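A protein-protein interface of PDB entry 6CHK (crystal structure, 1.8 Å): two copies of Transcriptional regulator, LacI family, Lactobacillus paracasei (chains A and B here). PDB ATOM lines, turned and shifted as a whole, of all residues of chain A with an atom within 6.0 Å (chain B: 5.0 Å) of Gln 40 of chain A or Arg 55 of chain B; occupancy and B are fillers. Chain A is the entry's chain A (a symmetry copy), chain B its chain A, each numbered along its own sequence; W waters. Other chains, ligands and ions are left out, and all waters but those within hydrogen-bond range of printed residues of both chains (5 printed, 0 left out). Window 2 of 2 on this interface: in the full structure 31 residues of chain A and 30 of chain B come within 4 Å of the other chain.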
ATOM      1  N   THR A   8       8.479 -20.573 -33.307  1.00  0.00           N
ATOM      2  CA  THR A   8       7.902 -19.719 -32.228  1.00  0.00           C
ATOM      3  C   THR A   8       8.888 -18.623 -31.819  1.00  0.00           C
ATOM      4  O   THR A   8       9.889 -18.909 -31.150  1.00  0.00           O
ATOM      5  CB  THR A   8       7.461 -20.545 -30.994  1.00  0.00           C
ATOM      6  OG1 THR A   8       8.588 -21.163 -30.359  1.00  0.00           O
ATOM      7  CG2 THR A   8       6.468 -21.619 -31.398  1.00  0.00           C
ATOM      8  N   GLY A   9       8.576 -17.388 -32.228  1.00  0.00           N
ATOM      9  CA  GLY A   9       9.469 -16.225 -32.132  1.00  0.00           C
ATOM     10  C   GLY A   9       9.225 -15.249 -30.973  1.00  0.00           C
ATOM     11  O   GLY A   9       9.170 -15.646 -29.819  1.00  0.00           O
ATOM     12  N   ASN A  10       9.114 -13.957 -31.308  1.00  0.00           N
ATOM     13  CA  ASN A  10       9.004 -12.862 -30.351  1.00  0.00           C
ATOM     14  C   ASN A  10       7.605 -12.256 -30.321  1.00  0.00           C
ATOM     15  O   ASN A  10       6.997 -12.009 -31.363  1.00  0.00           O
ATOM     16  CB  ASN A  10       9.990 -11.733 -30.727  1.00  0.00           C
ATOM     17  CG  ASN A  10      11.451 -12.157 -30.655  1.00  0.00           C
ATOM     18  OD1 ASN A  10      11.849 -13.015 -29.842  1.00  0.00           O
ATOM     19  ND2 ASN A  10      12.266 -11.533 -31.487  1.00  0.00           N
ATOM     20  N   ILE A  11       7.119 -11.967 -29.117  1.00  0.00           N
ATOM     21  CA  ILE A  11       5.844 -11.368 -28.904  1.00  0.00           C
ATOM     22  C   ILE A  11       6.076 -10.162 -28.010  1.00  0.00           C
ATOM     23  O   ILE A  11       6.817 -10.215 -27.010  1.00  0.00           O
ATOM     24  CB  ILE A  11       4.866 -12.308 -28.177  1.00  0.00           C
ATOM     25  CG1 ILE A  11       4.744 -13.670 -28.929  1.00  0.00           C
ATOM     26  CG2 ILE A  11       3.508 -11.696 -27.889  1.00  0.00           C
ATOM     27  CD1 ILE A  11       4.135 -13.624 -30.277  1.00  0.00           C
ATOM     28  N   GLY A  12       5.377  -9.106 -28.342  1.00  0.00           N
ATOM     29  CA  GLY A  12       5.392  -7.887 -27.543  1.00  0.00           C
ATOM     30  C   GLY A  12       4.094  -7.719 -26.766  1.00  0.00           C
ATOM     31  O   GLY A  12       3.005  -8.029 -27.265  1.00  0.00           O
ATOM     32  N   LEU A  34       3.100 -18.057 -22.730  1.00  0.00           N
ATOM     33  CA  LEU A  34       3.815 -17.989 -23.970  1.00  0.00           C
ATOM     34  C   LEU A  34       5.217 -18.572 -23.971  1.00  0.00           C
ATOM     35  O   LEU A  34       5.656 -19.223 -24.966  1.00  0.00           O
ATOM     36  CB  LEU A  34       3.843 -16.514 -24.490  1.00  0.00           C
ATOM     37  CG  LEU A  34       2.488 -16.022 -25.019  1.00  0.00           C
ATOM     38  CD1 LEU A  34       2.584 -14.527 -25.312  1.00  0.00           C
ATOM     39  CD2 LEU A  34       2.018 -16.764 -26.255  1.00  0.00           C
ATOM     40  N   HIS A  35       5.912 -18.374 -22.868  1.00  0.00           N
ATOM     41  CA  HIS A  35       7.217 -18.952 -22.685  1.00  0.00           C
ATOM     42  C   HIS A  35       7.142 -20.496 -22.781  1.00  0.00           C
ATOM     43  O   HIS A  35       7.937 -21.132 -23.428  1.00  0.00           O
ATOM     44  CB  HIS A  35       7.756 -18.570 -21.321  1.00  0.00           C
ATOM     45  CG  HIS A  35       9.044 -19.241 -20.992  1.00  0.00           C
ATOM     46  ND1 HIS A  35       9.126 -20.323 -20.141  1.00  0.00           N
ATOM     47  CD2 HIS A  35      10.295 -19.034 -21.471  1.00  0.00           C
ATOM     48  CE1 HIS A  35      10.382 -20.738 -20.096  1.00  0.00           C
ATOM     49  NE2 HIS A  35      11.107 -19.984 -20.909  1.00  0.00           N
ATOM     50  N   GLY A  38       7.213 -21.669 -26.229  1.00  0.00           N
ATOM     51  CA  GLY A  38       8.425 -21.449 -26.967  1.00  0.00           C
ATOM     52  C   GLY A  38       8.687 -20.015 -27.351  1.00  0.00           C
ATOM     53  O   GLY A  38       9.657 -19.737 -28.070  1.00  0.00           O
ATOM     54  N   TYR A  39       7.827 -19.098 -26.918  1.00  0.00           N
ATOM     55  CA  TYR A  39       8.016 -17.677 -27.326  1.00  0.00           C
ATOM     56  C   TYR A  39       8.817 -16.888 -26.302  1.00  0.00           C
ATOM     57  O   TYR A  39       8.780 -17.171 -25.108  1.00  0.00           O
ATOM     58  CB  TYR A  39       6.671 -16.968 -27.485  1.00  0.00           C
ATOM     59  CG  TYR A  39       5.895 -17.497 -28.627  1.00  0.00           C
ATOM     60  CD1 TYR A  39       6.053 -16.954 -29.868  1.00  0.00           C
ATOM     61  CD2 TYR A  39       4.992 -18.562 -28.455  1.00  0.00           C
ATOM     62  CE1 TYR A  39       5.342 -17.416 -30.952  1.00  0.00           C
ATOM     63  CE2 TYR A  39       4.283 -19.049 -29.526  1.00  0.00           C
ATOM     64  CZ  TYR A  39       4.483 -18.475 -30.776  1.00  0.00           C
ATOM     65  OH  TYR A  39       3.836 -18.893 -31.890  1.00  0.00           O
ATOM     66  N   GLN A  40       9.513 -15.867 -26.812  1.00  0.00           N
ATOM     67  CA  GLN A  40      10.184 -14.897 -25.984  1.00  0.00           C
ATOM     68  C   GLN A  40       9.260 -13.677 -25.960  1.00  0.00           C
ATOM     69  O   GLN A  40       8.838 -13.220 -27.021  1.00  0.00           O
ATOM     70  CB  GLN A  40      11.515 -14.500 -26.627  1.00  0.00           C
ATOM     71  CG  GLN A  40      12.286 -13.402 -25.908  1.00  0.00           C
ATOM     72  CD  GLN A  40      13.726 -13.369 -26.372  1.00  0.00           C
ATOM     73  OE1 GLN A  40      14.627 -13.457 -25.552  1.00  0.00           O
ATOM     74  NE2 GLN A  40      13.942 -13.322 -27.692  1.00  0.00           N
ATOM     75  N   VAL A  41       8.974 -13.156 -24.774  1.00  0.00           N
ATOM     76  CA  VAL A  41       7.937 -12.115 -24.648  1.00  0.00           C
ATOM     77  C   VAL A  41       8.593 -10.897 -23.986  1.00  0.00           C
ATOM     78  O   VAL A  41       9.345 -11.026 -23.031  1.00  0.00           O
ATOM     79  CB  VAL A  41       6.743 -12.583 -23.819  1.00  0.00           C
ATOM     80  CG1 VAL A  41       5.587 -11.609 -23.951  1.00  0.00           C
ATOM     81  CG2 VAL A  41       6.300 -13.964 -24.301  1.00  0.00           C
ATOM     82  N   MET A  42       8.319  -9.720 -24.529  1.00  0.00           N
ATOM     83  CA  MET A  42       8.935  -8.503 -24.000  1.00  0.00           C
ATOM     84  C   MET A  42       7.833  -7.468 -23.767  1.00  0.00           C
ATOM     85  O   MET A  42       6.852  -7.431 -24.498  1.00  0.00           O
ATOM     86  CB  MET A  42      10.055  -8.044 -24.971  1.00  0.00           C
ATOM     87  CG  MET A  42      11.054  -9.154 -25.372  1.00  0.00           C
ATOM     88  SD  MET A  42      10.657 -10.070 -26.888  1.00  0.00           S
ATOM     89  CE  MET A  42      11.052  -8.824 -28.121  1.00  0.00           C
ATOM     90  N   THR B  44      12.549  -8.064 -20.477  1.00  0.00           N
ATOM     91  CA  THR B  44      12.393  -9.538 -20.532  1.00  0.00           C
ATOM     92  C   THR B  44      12.662 -10.075 -19.127  1.00  0.00           C
ATOM     93  O   THR B  44      13.487  -9.536 -18.406  1.00  0.00           O
ATOM     94  CB  THR B  44      13.384 -10.082 -21.529  1.00  0.00           C
ATOM     95  OG1 THR B  44      12.981  -9.620 -22.834  1.00  0.00           O
ATOM     96  CG2 THR B  44      13.433 -11.616 -21.509  1.00  0.00           C
ATOM     97  N   GLU B  51      18.685 -20.398 -20.026  1.00  0.00           N
ATOM     98  CA  GLU B  51      18.268 -20.393 -21.428  1.00  0.00           C
ATOM     99  C   GLU B  51      17.515 -19.100 -21.837  1.00  0.00           C
ATOM    100  O   GLU B  51      17.655 -18.625 -22.991  1.00  0.00           O
ATOM    101  CB  GLU B  51      17.432 -21.621 -21.762  1.00  0.00           C
ATOM    102  CG  GLU B  51      18.255 -22.912 -21.636  1.00  0.00           C
ATOM    103  CD  GLU B  51      19.600 -22.866 -22.382  1.00  0.00           C
ATOM    104  OE1 GLU B  51      19.604 -22.992 -23.632  1.00  0.00           O
ATOM    105  OE2 GLU B  51      20.657 -22.713 -21.714  1.00  0.00           O
ATOM    106  N   ALA B  52      16.763 -18.552 -20.903  1.00  0.00           N
ATOM    107  CA  ALA B  52      16.079 -17.261 -21.156  1.00  0.00           C
ATOM    108  C   ALA B  52      17.099 -16.128 -21.312  1.00  0.00           C
ATOM    109  O   ALA B  52      16.961 -15.227 -22.161  1.00  0.00           O
ATOM    110  CB  ALA B  52      15.139 -16.935 -20.025  1.00  0.00           C
ATOM    111  N   GLU B  53      18.122 -16.162 -20.473  1.00  0.00           N
ATOM    112  CA  GLU B  53      19.242 -15.203 -20.597  1.00  0.00           C
ATOM    113  C   GLU B  53      19.951 -15.341 -21.939  1.00  0.00           C
ATOM    114  O   GLU B  53      20.198 -14.328 -22.641  1.00  0.00           O
ATOM    115  CB  GLU B  53      20.222 -15.383 -19.416  1.00  0.00           C
ATOM    116  CG  GLU B  53      21.519 -14.618 -19.511  1.00  0.00           C
ATOM    117  CD  GLU B  53      22.401 -14.872 -18.304  1.00  0.00           C
ATOM    118  OE1 GLU B  53      22.300 -14.128 -17.322  1.00  0.00           O
ATOM    119  OE2 GLU B  53      23.167 -15.851 -18.324  1.00  0.00           O
ATOM    120  N   GLU B  54      20.268 -16.585 -22.329  1.00  0.00           N
ATOM    121  CA  GLU B  54      20.886 -16.847 -23.617  1.00  0.00           C
ATOM    122  C   GLU B  54      20.063 -16.310 -24.769  1.00  0.00           C
ATOM    123  O   GLU B  54      20.578 -15.679 -25.709  1.00  0.00           O
ATOM    124  CB  GLU B  54      21.113 -18.360 -23.836  1.00  0.00           C
ATOM    125  CG  GLU B  54      21.886 -18.688 -25.109  1.00  0.00           C
ATOM    126  CD  GLU B  54      21.811 -20.173 -25.495  1.00  0.00           C
ATOM    127  OE1 GLU B  54      21.545 -21.028 -24.618  1.00  0.00           O
ATOM    128  OE2 GLU B  54      22.022 -20.501 -26.688  1.00  0.00           O
ATOM    129  N   ARG B  55      18.767 -16.566 -24.698  1.00  0.00           N
ATOM    130  CA  ARG B  55      17.878 -16.148 -25.767  1.00  0.00           C
ATOM    131  C   ARG B  55      17.794 -14.614 -25.914  1.00  0.00           C
ATOM    132  O   ARG B  55      17.782 -14.081 -27.028  1.00  0.00           O
ATOM    133  CB  ARG B  55      16.489 -16.675 -25.500  1.00  0.00           C
ATOM    134  CG  ARG B  55      15.653 -16.583 -26.744  1.00  0.00           C
ATOM    135  CD  ARG B  55      14.355 -17.328 -26.591  1.00  0.00           C
ATOM    136  NE  ARG B  55      13.608 -17.309 -27.848  1.00  0.00           N
ATOM    137  CZ  ARG B  55      12.449 -17.938 -28.040  1.00  0.00           C
ATOM    138  NH1 ARG B  55      11.890 -18.635 -27.051  1.00  0.00           N
ATOM    139  NH2 ARG B  55      11.828 -17.840 -29.217  1.00  0.00           N
ATOM    140  N   PHE B  56      17.789 -13.965 -24.771  1.00  0.00           N
ATOM    141  CA  PHE B  56      17.787 -12.488 -24.675  1.00  0.00           C
ATOM    142  C   PHE B  56      19.076 -11.942 -25.318  1.00  0.00           C
ATOM    143  O   PHE B  56      19.040 -11.030 -26.181  1.00  0.00           O
ATOM    144  CB  PHE B  56      17.694 -12.068 -23.225  1.00  0.00           C
ATOM    145  CG  PHE B  56      17.932 -10.566 -22.986  1.00  0.00           C
ATOM    146  CD1 PHE B  56      16.896  -9.657 -23.124  1.00  0.00           C
ATOM    147  CD2 PHE B  56      19.165 -10.111 -22.571  1.00  0.00           C
ATOM    148  CE1 PHE B  56      17.093  -8.298 -22.875  1.00  0.00           C
ATOM    149  CE2 PHE B  56      19.395  -8.742 -22.314  1.00  0.00           C
ATOM    150  CZ  PHE B  56      18.350  -7.841 -22.448  1.00  0.00           C
ATOM    151  N   LEU B  57      20.190 -12.549 -24.961  1.00  0.00           N
ATOM    152  CA  LEU B  57      21.472 -12.106 -25.528  1.00  0.00           C
ATOM    153  C   LEU B  57      21.544 -12.282 -27.039  1.00  0.00           C
ATOM    154  O   LEU B  57      22.251 -11.493 -27.683  1.00  0.00           O
ATOM    155  CB  LEU B  57      22.651 -12.767 -24.837  1.00  0.00           C
ATOM    156  CG  LEU B  57      22.810 -12.438 -23.344  1.00  0.00           C
ATOM    157  CD1 LEU B  57      23.813 -13.383 -22.726  1.00  0.00           C
ATOM    158  CD2 LEU B  57      23.176 -10.996 -23.085  1.00  0.00           C
ATOM    159  N   LYS B  58      20.856 -13.292 -27.623  1.00  0.00           N
ATOM    160  CA  LYS B  58      20.800 -13.428 -29.069  1.00  0.00           C
ATOM    161  C   LYS B  58      20.203 -12.227 -29.758  1.00  0.00           C
ATOM    162  O   LYS B  58      20.610 -11.904 -30.879  1.00  0.00           O
ATOM    163  CB  LYS B  58      20.019 -14.689 -29.495  1.00  0.00           C
ATOM    164  CG  LYS B  58      20.711 -15.978 -29.115  1.00  0.00           C
ATOM    165  CD  LYS B  58      19.901 -17.153 -29.618  1.00  0.00           C
ATOM    166  CE  LYS B  58      20.591 -18.467 -29.288  1.00  0.00           C
ATOM    167  NZ  LYS B  58      19.761 -19.567 -29.825  1.00  0.00           N
ATOM    168  N   GLN B  59      19.305 -11.507 -29.078  1.00  0.00           N
ATOM    169  CA  GLN B  59      18.755 -10.274 -29.659  1.00  0.00           C
ATOM    170  C   GLN B  59      19.831  -9.173 -29.868  1.00  0.00           C
ATOM    171  O   GLN B  59      19.751  -8.397 -30.805  1.00  0.00           O
ATOM    172  CB  GLN B  59      17.651  -9.723 -28.804  1.00  0.00           C
ATOM    173  CG  GLN B  59      16.463 -10.663 -28.608  1.00  0.00           C
ATOM    174  CD  GLN B  59      15.332  -9.915 -27.955  1.00  0.00           C
ATOM    175  OE1 GLN B  59      15.338  -9.745 -26.744  1.00  0.00           O
ATOM    176  NE2 GLN B  59      14.384  -9.404 -28.765  1.00  0.00           N
HETATM  177  O   HOH W   1      12.864 -15.552 -30.686  1.00  0.00           O
HETATM  178  O   HOH W   2      16.407 -14.176 -29.296  1.00  0.00           O
HETATM  179  O   HOH W   3      13.903 -20.404 -20.994  1.00  0.00           O
HETATM  180  O   HOH W   4      14.092 -10.836 -24.946  1.00  0.00           O
HETATM  181  O   HOH W   5      14.492 -14.726 -23.179  1.00  0.00           O
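O of Gly 38 of chain A is in hydrogen-bond range of NH1 of Arg 55 of chain B, at 2.7 Å.
The side-chain amide oxygen of Gln 40 of chain A sits at hydrogen-bond distance from the backbone NH of Phe 56 of chain B (3.3 Å).
The guanidinium group (NH2) of Arg 55 of chain B is in hydrogen-bond range of the backbone carbonyl oxygen (O) of Thr 8 of chain A (2.9 Å).
NH2 of Arg 55 of chain B sits at hydrogen-bond distance from O of Gly 9 of chain A.
The backbone carbonyl oxygen of Leu 34 of chain A is in hydrogen-bond range of the backbone NH of Tyr 39 of chain A, 2.9 Å away.
The side-chain amide nitrogen of Gln 40 of chain A lies within hydrogen-bond range of the side-chain amide oxygen of Asn 10 of chain A (3.0 Å).
The side-chain hydroxyl (OG1) of Thr 8 of chain A is in hydrogen-bond range of the backbone carbonyl oxygen (O) of Gly 38 of chain A (2.9 Å).
The backbone carbonyl oxygen (O) of Ile 11 of chain A lies within hydrogen-bond range of the backbone NH (N) of Met 42 of chain A (2.9 Å).
The backbone carbonyl oxygen (O) of Gln 40 of chain A sits at hydrogen-bond distance from the backbone NH (N) of Ile 11 of chain A (3.0 Å).
The backbone carbonyl oxygen of Gly 9 of chain A sits at hydrogen-bond distance from the backbone NH of Gln 40 of chain A.
Tyr 39 of chain A touches Arg 55 of chain B.
OE1 of Gln 40 of chain A touches C of Arg 55 of chain B, 3.4 Å away.
Gln 40 of chain A touches Gln 59 of chain B (NE2 to CD, 3.7 Å).
O of Val 41 of chain A touches OG1 of Thr 44 of chain B, at 3.9 Å.
CG of Met 42 of chain A touches OG1 of Thr 44 of chain B, at 3.2 Å.
Met 42 of chain A touches Gln 59 of chain B.
Of chain B, only Arg 55 (3.4 Å), Phe 56 (3.3 Å) and Gln 59 (3.7 Å) come within 4 Å of Gln 40 of chain A.
Arg 55 of chain B touches just these residues of chain A: Thr 8 (2.9 Å), Gly 9 (3.5 Å), Gly 38 (2.7 Å), Tyr 39 (3.6 Å) and Gln 40 (3.4 Å).
Printed residues of chain B within 4 Å of Gly 38 of chain A: Arg 55 (2.7 Å).
Of the printed residues of chain B, Val 41 of chain A touches Thr 44.
Glu 53 of chain B touches none of the printed residues of chain A.
Ala 52 of chain B touches none of the printed residues of chain A.
Hydrophobic or aromatic side chains of chain A within 4 Å of the printed part of chain B: Met 42.
Printed residues of chain B that touch a printed residue of chain A: Thr 44, Arg 55, Phe 56 and Gln 59.
No position is printed for both chains.
Of the 10 pairs that touch across the chains among the printed residues, none has its exchanged pair printed and touching as well.
Water W4 lies within hydrogen-bond range of the side-chain amide oxygen (OE1) of Gln 59 of chain B (2.4 Å), the side-chain hydroxyl (OG1) of Thr 44 of chain B (2.7 Å) and the side-chain amide oxygen (OE1) of Gln 40 of chain A (2.7 Å).
Water W2 lies within hydrogen-bond range of the backbone carbonyl oxygen of Arg 55 of chain B (2.7 Å) and the side-chain amide nitrogen of Gln 40 of chain A (3.1 Å).
Water W5 bridges OE1 of Gln 40 of chain A and O of Ala 52 of chain B.
Water W3 lies within hydrogen-bond range of NE2 of His 35 of chain A (2.8 Å) and N of Ala 52 of chain B (3.4 Å).
Water W1 bridges the side-chain amide oxygen of Asn 10 of chain A (2.9 Å) and the guanidinium group of Arg 55 of chain B (2.9 Å).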
